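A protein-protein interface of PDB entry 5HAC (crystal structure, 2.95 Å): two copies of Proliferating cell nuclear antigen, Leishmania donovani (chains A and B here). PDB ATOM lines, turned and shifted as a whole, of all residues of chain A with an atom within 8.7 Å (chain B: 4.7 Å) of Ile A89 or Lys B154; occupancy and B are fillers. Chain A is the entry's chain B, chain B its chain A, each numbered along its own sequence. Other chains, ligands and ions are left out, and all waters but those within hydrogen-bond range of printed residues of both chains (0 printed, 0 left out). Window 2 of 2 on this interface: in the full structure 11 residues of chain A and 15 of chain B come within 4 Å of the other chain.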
ATOM      1  N   ALA A  17      14.419  -6.420   5.707  1.00  0.00           N
ATOM      2  CA  ALA A  17      14.750  -7.534   4.759  1.00  0.00           C
ATOM      3  C   ALA A  17      16.222  -7.649   4.398  1.00  0.00           C
ATOM      4  O   ALA A  17      16.679  -8.684   3.943  1.00  0.00           O
ATOM      5  CB  ALA A  17      13.939  -7.410   3.469  1.00  0.00           C
ATOM      6  N   LYS A  21      18.519 -10.918   2.809  1.00  0.00           N
ATOM      7  CA  LYS A  21      19.278 -10.669   1.603  1.00  0.00           C
ATOM      8  C   LYS A  21      20.717 -11.018   1.868  1.00  0.00           C
ATOM      9  O   LYS A  21      21.269 -11.894   1.209  1.00  0.00           O
ATOM     10  CB  LYS A  21      19.141  -9.208   1.186  1.00  0.00           C
ATOM     11  CG  LYS A  21      17.762  -8.840   0.648  1.00  0.00           C
ATOM     12  CD  LYS A  21      17.583  -7.342   0.441  1.00  0.00           C
ATOM     13  CE  LYS A  21      18.432  -6.765  -0.689  1.00  0.00           C
ATOM     14  NZ  LYS A  21      17.979  -7.232  -2.033  1.00  0.00           N
ATOM     15  N   SER A  82      17.246 -19.749  -6.513  1.00  0.00           N
ATOM     16  CA  SER A  82      15.964 -19.057  -6.626  1.00  0.00           C
ATOM     17  C   SER A  82      15.706 -18.069  -5.503  1.00  0.00           C
ATOM     18  O   SER A  82      15.306 -16.919  -5.736  1.00  0.00           O
ATOM     19  CB  SER A  82      14.801 -20.031  -6.584  1.00  0.00           C
ATOM     20  OG  SER A  82      14.959 -21.021  -7.562  1.00  0.00           O
ATOM     21  N   LEU A  83      15.889 -18.519  -4.272  1.00  0.00           N
ATOM     22  CA  LEU A  83      15.655 -17.637  -3.138  1.00  0.00           C
ATOM     23  C   LEU A  83      16.495 -16.357  -3.267  1.00  0.00           C
ATOM     24  O   LEU A  83      15.984 -15.259  -3.045  1.00  0.00           O
ATOM     25  CB  LEU A  83      15.986 -18.339  -1.835  1.00  0.00           C
ATOM     26  CG  LEU A  83      15.672 -17.548  -0.573  1.00  0.00           C
ATOM     27  CD1 LEU A  83      14.186 -17.347  -0.413  1.00  0.00           C
ATOM     28  CD2 LEU A  83      16.257 -18.250   0.642  1.00  0.00           C
ATOM     29  N   SER A  84      17.764 -16.508  -3.653  1.00  0.00           N
ATOM     30  CA  SER A  84      18.627 -15.357  -3.887  1.00  0.00           C
ATOM     31  C   SER A  84      18.033 -14.454  -4.973  1.00  0.00           C
ATOM     32  O   SER A  84      17.963 -13.251  -4.795  1.00  0.00           O
ATOM     33  CB  SER A  84      20.065 -15.771  -4.248  1.00  0.00           C
ATOM     34  OG  SER A  84      20.951 -14.682  -3.997  1.00  0.00           O
ATOM     35  N   LYS A  85      17.596 -15.039  -6.091  1.00  0.00           N
ATOM     36  CA  LYS A  85      16.959 -14.277  -7.192  1.00  0.00           C
ATOM     37  C   LYS A  85      15.772 -13.426  -6.747  1.00  0.00           C
ATOM     38  O   LYS A  85      15.618 -12.309  -7.200  1.00  0.00           O
ATOM     39  CB  LYS A  85      16.539 -15.198  -8.340  1.00  0.00           C
ATOM     40  CG  LYS A  85      17.722 -15.654  -9.151  1.00  0.00           C
ATOM     41  CD  LYS A  85      17.375 -16.742 -10.148  1.00  0.00           C
ATOM     42  CE  LYS A  85      18.652 -17.452 -10.584  1.00  0.00           C
ATOM     43  NZ  LYS A  85      18.334 -18.710 -11.296  1.00  0.00           N
ATOM     44  N   VAL A  86      14.981 -13.956  -5.838  1.00  0.00           N
ATOM     45  CA  VAL A  86      13.865 -13.236  -5.295  1.00  0.00           C
ATOM     46  C   VAL A  86      14.320 -12.182  -4.307  1.00  0.00           C
ATOM     47  O   VAL A  86      13.868 -11.051  -4.340  1.00  0.00           O
ATOM     48  CB  VAL A  86      12.869 -14.196  -4.608  1.00  0.00           C
ATOM     49  CG1 VAL A  86      11.722 -13.445  -3.965  1.00  0.00           C
ATOM     50  CG2 VAL A  86      12.324 -15.152  -5.644  1.00  0.00           C
ATOM     51  N   LEU A  87      15.196 -12.536  -3.396  1.00  0.00           N
ATOM     52  CA  LEU A  87      15.642 -11.554  -2.430  1.00  0.00           C
ATOM     53  C   LEU A  87      16.380 -10.391  -3.095  1.00  0.00           C
ATOM     54  O   LEU A  87      16.310  -9.266  -2.611  1.00  0.00           O
ATOM     55  CB  LEU A  87      16.488 -12.200  -1.348  1.00  0.00           C
ATOM     56  CG  LEU A  87      15.675 -13.188  -0.503  1.00  0.00           C
ATOM     57  CD1 LEU A  87      16.604 -14.058   0.300  1.00  0.00           C
ATOM     58  CD2 LEU A  87      14.721 -12.478   0.424  1.00  0.00           C
ATOM     59  N   LYS A  88      17.040 -10.645  -4.220  1.00  0.00           N
ATOM     60  CA  LYS A  88      17.727  -9.575  -4.950  1.00  0.00           C
ATOM     61  C   LYS A  88      16.774  -8.450  -5.307  1.00  0.00           C
ATOM     62  O   LYS A  88      17.153  -7.300  -5.253  1.00  0.00           O
ATOM     63  CB  LYS A  88      18.506 -10.083  -6.193  1.00  0.00           C
ATOM     64  CG  LYS A  88      20.016 -10.304  -5.891  1.00  0.00           C
ATOM     65  CD  LYS A  88      20.546 -11.367  -4.882  1.00  0.00           C
ATOM     66  CE  LYS A  88      19.945 -11.357  -3.438  1.00  0.00           C
ATOM     67  NZ  LYS A  88      20.589 -10.543  -2.365  1.00  0.00           N
ATOM     68  N   ILE A  89      15.516  -8.775  -5.594  1.00  0.00           N
ATOM     69  CA  ILE A  89      14.524  -7.751  -5.928  1.00  0.00           C
ATOM     70  C   ILE A  89      13.754  -7.127  -4.754  1.00  0.00           C
ATOM     71  O   ILE A  89      12.917  -6.283  -4.987  1.00  0.00           O
ATOM     72  CB  ILE A  89      13.478  -8.258  -6.937  1.00  0.00           C
ATOM     73  CG1 ILE A  89      12.585  -9.335  -6.343  1.00  0.00           C
ATOM     74  CG2 ILE A  89      14.163  -8.736  -8.197  1.00  0.00           C
ATOM     75  CD1 ILE A  89      11.351  -9.607  -7.172  1.00  0.00           C
ATOM     76  N   VAL A  90      14.029  -7.520  -3.522  1.00  0.00           N
ATOM     77  CA  VAL A  90      13.272  -7.032  -2.383  1.00  0.00           C
ATOM     78  C   VAL A  90      14.029  -5.878  -1.785  1.00  0.00           C
ATOM     79  O   VAL A  90      15.201  -6.026  -1.470  1.00  0.00           O
ATOM     80  CB  VAL A  90      13.108  -8.113  -1.311  1.00  0.00           C
ATOM     81  CG1 VAL A  90      12.460  -7.546  -0.071  1.00  0.00           C
ATOM     82  CG2 VAL A  90      12.257  -9.221  -1.861  1.00  0.00           C
ATOM     83  N   ASP A  91      13.348  -4.759  -1.550  1.00  0.00           N
ATOM     84  CA  ASP A  91      14.000  -3.588  -0.969  1.00  0.00           C
ATOM     85  C   ASP A  91      14.534  -3.917   0.430  1.00  0.00           C
ATOM     86  O   ASP A  91      13.841  -4.463   1.263  1.00  0.00           O
ATOM     87  CB  ASP A  91      13.053  -2.396  -0.914  1.00  0.00           C
ATOM     88  CG  ASP A  91      13.733  -1.103  -0.456  1.00  0.00           C
ATOM     89  OD1 ASP A  91      14.914  -1.095  -0.068  1.00  0.00           O
ATOM     90  OD2 ASP A  91      13.057  -0.066  -0.443  1.00  0.00           O
ATOM     91  N   SER A  92      15.818  -3.640   0.613  1.00  0.00           N
ATOM     92  CA  SER A  92      16.526  -3.634   1.910  1.00  0.00           C
ATOM     93  C   SER A  92      15.670  -3.241   3.118  1.00  0.00           C
ATOM     94  O   SER A  92      15.654  -3.969   4.106  1.00  0.00           O
ATOM     95  CB  SER A  92      17.777  -2.663   1.857  1.00  0.00           C
ATOM     96  OG  SER A  92      18.777  -2.983   0.856  1.00  0.00           O
ATOM     97  N   ASP A  94      12.301  -2.710   3.369  1.00  0.00           N
ATOM     98  CA  ASP A  94      10.999  -3.308   3.545  1.00  0.00           C
ATOM     99  C   ASP A  94      11.047  -4.430   4.613  1.00  0.00           C
ATOM    100  O   ASP A  94      12.096  -5.026   4.886  1.00  0.00           O
ATOM    101  CB  ASP A  94      10.462  -3.815   2.196  1.00  0.00           C
ATOM    102  CG  ASP A  94      10.036  -2.672   1.261  1.00  0.00           C
ATOM    103  OD1 ASP A  94      10.193  -1.481   1.644  1.00  0.00           O
ATOM    104  OD2 ASP A  94       9.550  -2.988   0.135  1.00  0.00           O
ATOM    105  N   SER A 111       6.538  -8.979   1.499  1.00  0.00           N
ATOM    106  CA  SER A 111       7.290  -7.779   1.765  1.00  0.00           C
ATOM    107  C   SER A 111       6.331  -6.623   1.776  1.00  0.00           C
ATOM    108  O   SER A 111       5.372  -6.575   0.991  1.00  0.00           O
ATOM    109  CB  SER A 111       8.361  -7.555   0.682  1.00  0.00           C
ATOM    110  OG  SER A 111       8.334  -6.228   0.162  1.00  0.00           O
ATOM    111  N   ASN A 113       6.433  -2.138   2.519  1.00  0.00           N
ATOM    112  CA  ASN A 113       6.966  -0.844   2.929  1.00  0.00           C
ATOM    113  C   ASN A 113       6.727  -0.480   4.372  1.00  0.00           C
ATOM    114  O   ASN A 113       5.705  -0.875   4.920  1.00  0.00           O
ATOM    115  CB  ASN A 113       6.033   0.230   2.331  1.00  0.00           C
ATOM    116  CG  ASN A 113       6.336   0.623   0.946  1.00  0.00           C
ATOM    117  OD1 ASN A 113       7.374   0.317   0.413  1.00  0.00           O
ATOM    118  ND2 ASN A 113       5.432   1.389   0.363  1.00  0.00           N
ATOM    119  N   ARG A 118       2.835  -0.249  -0.700  1.00  0.00           N
ATOM    120  CA  ARG A 118       3.274  -1.309  -1.607  1.00  0.00           C
ATOM    121  C   ARG A 118       3.314  -2.611  -0.834  1.00  0.00           C
ATOM    122  O   ARG A 118       3.770  -2.649   0.303  1.00  0.00           O
ATOM    123  CB  ARG A 118       4.668  -1.007  -2.193  1.00  0.00           C
ATOM    124  CG  ARG A 118       5.408  -2.221  -2.790  1.00  0.00           C
ATOM    125  CD  ARG A 118       6.529  -1.859  -3.767  1.00  0.00           C
ATOM    126  NE  ARG A 118       7.871  -2.067  -3.215  1.00  0.00           N
ATOM    127  CZ  ARG A 118       8.718  -1.122  -2.801  1.00  0.00           C
ATOM    128  NH1 ARG A 118       8.412   0.163  -2.848  1.00  0.00           N
ATOM    129  NH2 ARG A 118       9.917  -1.469  -2.334  1.00  0.00           N
ATOM    130  N   CYS A 120       4.405  -6.811  -1.656  1.00  0.00           N
ATOM    131  CA  CYS A 120       4.936  -7.786  -2.583  1.00  0.00           C
ATOM    132  C   CYS A 120       4.773  -9.153  -2.006  1.00  0.00           C
ATOM    133  O   CYS A 120       4.901  -9.323  -0.799  1.00  0.00           O
ATOM    134  CB  CYS A 120       6.394  -7.523  -2.816  1.00  0.00           C
ATOM    135  SG  CYS A 120       6.609  -5.995  -3.724  1.00  0.00           S
ATOM    136  N   GLU A 121       4.455 -10.127  -2.862  1.00  0.00           N
ATOM    137  CA  GLU A 121       4.349 -11.507  -2.411  1.00  0.00           C
ATOM    138  C   GLU A 121       4.826 -12.528  -3.422  1.00  0.00           C
ATOM    139  O   GLU A 121       4.256 -12.713  -4.502  1.00  0.00           O
ATOM    140  CB  GLU A 121       2.935 -11.849  -1.969  1.00  0.00           C
ATOM    141  CG  GLU A 121       2.890 -13.076  -1.084  1.00  0.00           C
ATOM    142  CD  GLU A 121       1.481 -13.489  -0.788  1.00  0.00           C
ATOM    143  OE1 GLU A 121       0.946 -13.022   0.258  1.00  0.00           O
ATOM    144  OE2 GLU A 121       0.912 -14.241  -1.629  1.00  0.00           O
ATOM    145  N   TYR A 122       5.869 -13.221  -3.008  1.00  0.00           N
ATOM    146  CA  TYR A 122       6.548 -14.186  -3.823  1.00  0.00           C
ATOM    147  C   TYR A 122       6.321 -15.568  -3.228  1.00  0.00           C
ATOM    148  O   TYR A 122       6.328 -15.725  -2.009  1.00  0.00           O
ATOM    149  CB  TYR A 122       8.039 -13.822  -3.872  1.00  0.00           C
ATOM    150  CG  TYR A 122       8.284 -12.354  -4.164  1.00  0.00           C
ATOM    151  CD1 TYR A 122       8.033 -11.822  -5.424  1.00  0.00           C
ATOM    152  CD2 TYR A 122       8.747 -11.483  -3.176  1.00  0.00           C
ATOM    153  CE1 TYR A 122       8.239 -10.462  -5.696  1.00  0.00           C
ATOM    154  CE2 TYR A 122       8.975 -10.114  -3.443  1.00  0.00           C
ATOM    155  CZ  TYR A 122       8.728  -9.597  -4.701  1.00  0.00           C
ATOM    156  OH  TYR A 122       8.901  -8.240  -4.975  1.00  0.00           O
ATOM    157  N   ALA B 150      10.164   5.372 -11.948  1.00  0.00           N
ATOM    158  CA  ALA B 150      11.198   4.469 -11.510  1.00  0.00           C
ATOM    159  C   ALA B 150      10.686   3.251 -10.762  1.00  0.00           C
ATOM    160  O   ALA B 150      11.323   2.193 -10.833  1.00  0.00           O
ATOM    161  CB  ALA B 150      12.204   5.201 -10.652  1.00  0.00           C
ATOM    162  N   GLU B 151       9.579   3.381 -10.046  1.00  0.00           N
ATOM    163  CA  GLU B 151       8.946   2.230  -9.363  1.00  0.00           C
ATOM    164  C   GLU B 151       8.473   1.285 -10.448  1.00  0.00           C
ATOM    165  O   GLU B 151       8.646   0.072 -10.372  1.00  0.00           O
ATOM    166  CB  GLU B 151       7.759   2.634  -8.452  1.00  0.00           C
ATOM    167  CG  GLU B 151       7.054   1.487  -7.699  1.00  0.00           C
ATOM    168  CD  GLU B 151       7.940   0.757  -6.694  1.00  0.00           C
ATOM    169  OE1 GLU B 151       8.801   1.416  -6.072  1.00  0.00           O
ATOM    170  OE2 GLU B 151       7.770  -0.482  -6.492  1.00  0.00           O
ATOM    171  N   PHE B 152       7.868   1.876 -11.464  1.00  0.00           N
ATOM    172  CA  PHE B 152       7.395   1.121 -12.589  1.00  0.00           C
ATOM    173  C   PHE B 152       8.545   0.332 -13.174  1.00  0.00           C
ATOM    174  O   PHE B 152       8.426  -0.871 -13.390  1.00  0.00           O
ATOM    175  CB  PHE B 152       6.795   2.060 -13.648  1.00  0.00           C
ATOM    176  CG  PHE B 152       6.369   1.345 -14.886  1.00  0.00           C
ATOM    177  CD1 PHE B 152       5.373   0.357 -14.806  1.00  0.00           C
ATOM    178  CD2 PHE B 152       6.967   1.618 -16.113  1.00  0.00           C
ATOM    179  CE1 PHE B 152       4.970  -0.337 -15.934  1.00  0.00           C
ATOM    180  CE2 PHE B 152       6.562   0.939 -17.249  1.00  0.00           C
ATOM    181  CZ  PHE B 152       5.557  -0.041 -17.158  1.00  0.00           C
ATOM    182  N   ALA B 153       9.660   1.022 -13.404  1.00  0.00           N
ATOM    183  CA  ALA B 153      10.850   0.405 -13.993  1.00  0.00           C
ATOM    184  C   ALA B 153      11.311  -0.762 -13.165  1.00  0.00           C
ATOM    185  O   ALA B 153      11.552  -1.827 -13.733  1.00  0.00           O
ATOM    186  CB  ALA B 153      11.988   1.406 -14.150  1.00  0.00           C
ATOM    187  N   LYS B 154      11.420  -0.547 -11.845  1.00  0.00           N
ATOM    188  CA  LYS B 154      11.779  -1.601 -10.874  1.00  0.00           C
ATOM    189  C   LYS B 154      10.827  -2.776 -11.018  1.00  0.00           C
ATOM    190  O   LYS B 154      11.242  -3.896 -11.282  1.00  0.00           O
ATOM    191  CB  LYS B 154      11.759  -1.079  -9.427  1.00  0.00           C
ATOM    192  CG  LYS B 154      12.408  -1.987  -8.380  1.00  0.00           C
ATOM    193  CD  LYS B 154      11.674  -1.959  -7.025  1.00  0.00           C
ATOM    194  CE  LYS B 154      12.506  -2.427  -5.833  1.00  0.00           C
ATOM    195  NZ  LYS B 154      13.324  -3.638  -6.160  1.00  0.00           N
ATOM    196  N   ILE B 155       9.544  -2.495 -10.922  1.00  0.00           N
ATOM    197  CA  ILE B 155       8.540  -3.534 -11.010  1.00  0.00           C
ATOM    198  C   ILE B 155       8.675  -4.424 -12.242  1.00  0.00           C
ATOM    199  O   ILE B 155       8.573  -5.645 -12.124  1.00  0.00           O
ATOM    200  CB  ILE B 155       7.126  -2.954 -10.948  1.00  0.00           C
ATOM    201  CG1 ILE B 155       6.840  -2.485  -9.530  1.00  0.00           C
ATOM    202  CG2 ILE B 155       6.079  -4.001 -11.338  1.00  0.00           C
ATOM    203  CD1 ILE B 155       5.619  -1.608  -9.442  1.00  0.00           C
ATOM    204  N   VAL B 156       8.902  -3.848 -13.418  1.00  0.00           N
ATOM    205  CA  VAL B 156       9.094  -4.660 -14.595  1.00  0.00           C
ATOM    206  C   VAL B 156      10.364  -5.554 -14.398  1.00  0.00           C
ATOM    207  O   VAL B 156      10.262  -6.787 -14.404  1.00  0.00           O
ATOM    208  CB  VAL B 156       9.252  -3.728 -15.815  1.00  0.00           C
ATOM    209  CG1 VAL B 156       9.505  -4.521 -17.066  1.00  0.00           C
ATOM    210  CG2 VAL B 156       8.134  -2.708 -16.061  1.00  0.00           C
ATOM    211  N   ARG B 157      11.522  -4.945 -14.155  1.00  0.00           N
ATOM    212  CA  ARG B 157      12.797  -5.658 -13.895  1.00  0.00           C
ATOM    213  C   ARG B 157      12.616  -6.814 -12.891  1.00  0.00           C
ATOM    214  O   ARG B 157      13.124  -7.937 -13.094  1.00  0.00           O
ATOM    215  CB  ARG B 157      13.837  -4.668 -13.350  1.00  0.00           C
ATOM    216  CG  ARG B 157      15.291  -5.089 -13.505  1.00  0.00           C
ATOM    217  CD  ARG B 157      16.253  -4.079 -12.884  1.00  0.00           C
ATOM    218  NE  ARG B 157      15.784  -2.678 -13.026  1.00  0.00           N
ATOM    219  CZ  ARG B 157      15.354  -1.885 -12.040  1.00  0.00           C
ATOM    220  NH1 ARG B 157      15.316  -2.304 -10.768  1.00  0.00           N
ATOM    221  NH2 ARG B 157      14.952  -0.644 -12.322  1.00  0.00           N
ATOM    222  N   ASP B 158      11.900  -6.508 -11.812  1.00  0.00           N
ATOM    223  CA  ASP B 158      11.507  -7.487 -10.814  1.00  0.00           C
ATOM    224  C   ASP B 158      10.720  -8.635 -11.431  1.00  0.00           C
ATOM    225  O   ASP B 158      11.181  -9.759 -11.406  1.00  0.00           O
ATOM    226  CB  ASP B 158      10.685  -6.847  -9.681  1.00  0.00           C
ATOM    227  CG  ASP B 158      11.522  -5.946  -8.770  1.00  0.00           C
ATOM    228  OD1 ASP B 158      12.724  -5.651  -9.088  1.00  0.00           O
ATOM    229  OD2 ASP B 158      10.974  -5.572  -7.707  1.00  0.00           O
ATOM    230  N   VAL B 161      12.269 -11.695 -13.283  1.00  0.00           N
ATOM    231  CA  VAL B 161      12.980 -12.829 -12.651  1.00  0.00           C
ATOM    232  C   VAL B 161      12.143 -14.079 -12.740  1.00  0.00           C
ATOM    233  O   VAL B 161      12.692 -15.182 -12.673  1.00  0.00           O
ATOM    234  CB  VAL B 161      13.406 -12.652 -11.153  1.00  0.00           C
ATOM    235  CG1 VAL B 161      14.210 -11.369 -10.923  1.00  0.00           C
ATOM    236  CG2 VAL B 161      12.220 -12.750 -10.210  1.00  0.00           C
ATOM    237  N   PHE B 162      10.825 -13.890 -12.843  1.00  0.00           N
ATOM    238  CA  PHE B 162       9.867 -14.994 -12.904  1.00  0.00           C
ATOM    239  C   PHE B 162       9.580 -15.429 -14.320  1.00  0.00           C
ATOM    240  O   PHE B 162       9.920 -16.543 -14.678  1.00  0.00           O
ATOM    241  CB  PHE B 162       8.584 -14.630 -12.172  1.00  0.00           C
ATOM    242  CG  PHE B 162       8.824 -14.292 -10.746  1.00  0.00           C
ATOM    243  CD1 PHE B 162       8.979 -15.290  -9.824  1.00  0.00           C
ATOM    244  CD2 PHE B 162       8.978 -12.978 -10.344  1.00  0.00           C
ATOM    245  CE1 PHE B 162       9.249 -14.988  -8.498  1.00  0.00           C
ATOM    246  CE2 PHE B 162       9.251 -12.664  -9.021  1.00  0.00           C
ATOM    247  CZ  PHE B 162       9.387 -13.671  -8.094  1.00  0.00           C
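Of the printed residues of chain B, Ile A89 touches Lys B154 (2.9 Å), Asp B158 (3.4 Å) and Val B161 (3.8 Å). Lys B154 touches just one residue of chain A: Ile A89. No residue of chain A comes within 4 Å of Ala B153. Of chain A, only Ile A89 (3.4 Å) comes within 4 Å of Asp B158. Of the printed residues of chain A, Phe B162 touches Tyr A122 (3.5 Å). Printed residues of chain B within 4 Å of Arg A118: Glu B151 (3.3 Å). Asp A94 touches none of the printed residues of chain B. Ile B155 touches none of the printed residues of chain A. The nearest residue of chain B that does not touch Ile A89 is Phe B162 (4.1 Å). The nearest printed residue of chain B that does not touch Tyr A122 is Asp B158 (4.3 Å).
The side-chain carboxylate (OD2) of Asp A91 is in salt-bridge range of the guanidinium group (NH2) of Arg A118. The side-chain carboxylate of Asp A94 lies within salt-bridge range of the guanidinium group of Arg A118 (2.9 Å). The side-chain amide nitrogen of Asn A113 sits close to the backbone NH of Arg A118 (3.2 Å). OH of Tyr A122 sits close to SG of Cys A120. NZ of Lys B154 lies within salt-bridge range of OD2 of Asp B158, at 3.4 Å.
Among the printed residues, pairs that only touch across the chains: Tyr A122 with Phe B162 (3.5 Å) and Ile A89 with Val B161 (3.8 Å).
No position is printed for both chains.
Hydrophobic or aromatic side chains of chain B within 4 Å of the printed part of chain A: Val B161 and Phe B162. Of the 20 printed residues of chain A, 3 touch a printed residue of chain B. Printed residues of chain A that touch a printed residue of chain B: Ile A89, Arg A118 and Tyr A122.
The side-chain carboxylate (OD2) of Asp B158 lies close to the backbone carbonyl oxygen (O) of Ile A89, 3.4 Å away. The side-chain carboxylate of Glu B151 is in salt-bridge range of the guanidinium group of Arg A118, at 3.5 Å. NZ of Lys B154 is in hydrogen-bond range of O of Ile A89 (2.9 Å).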
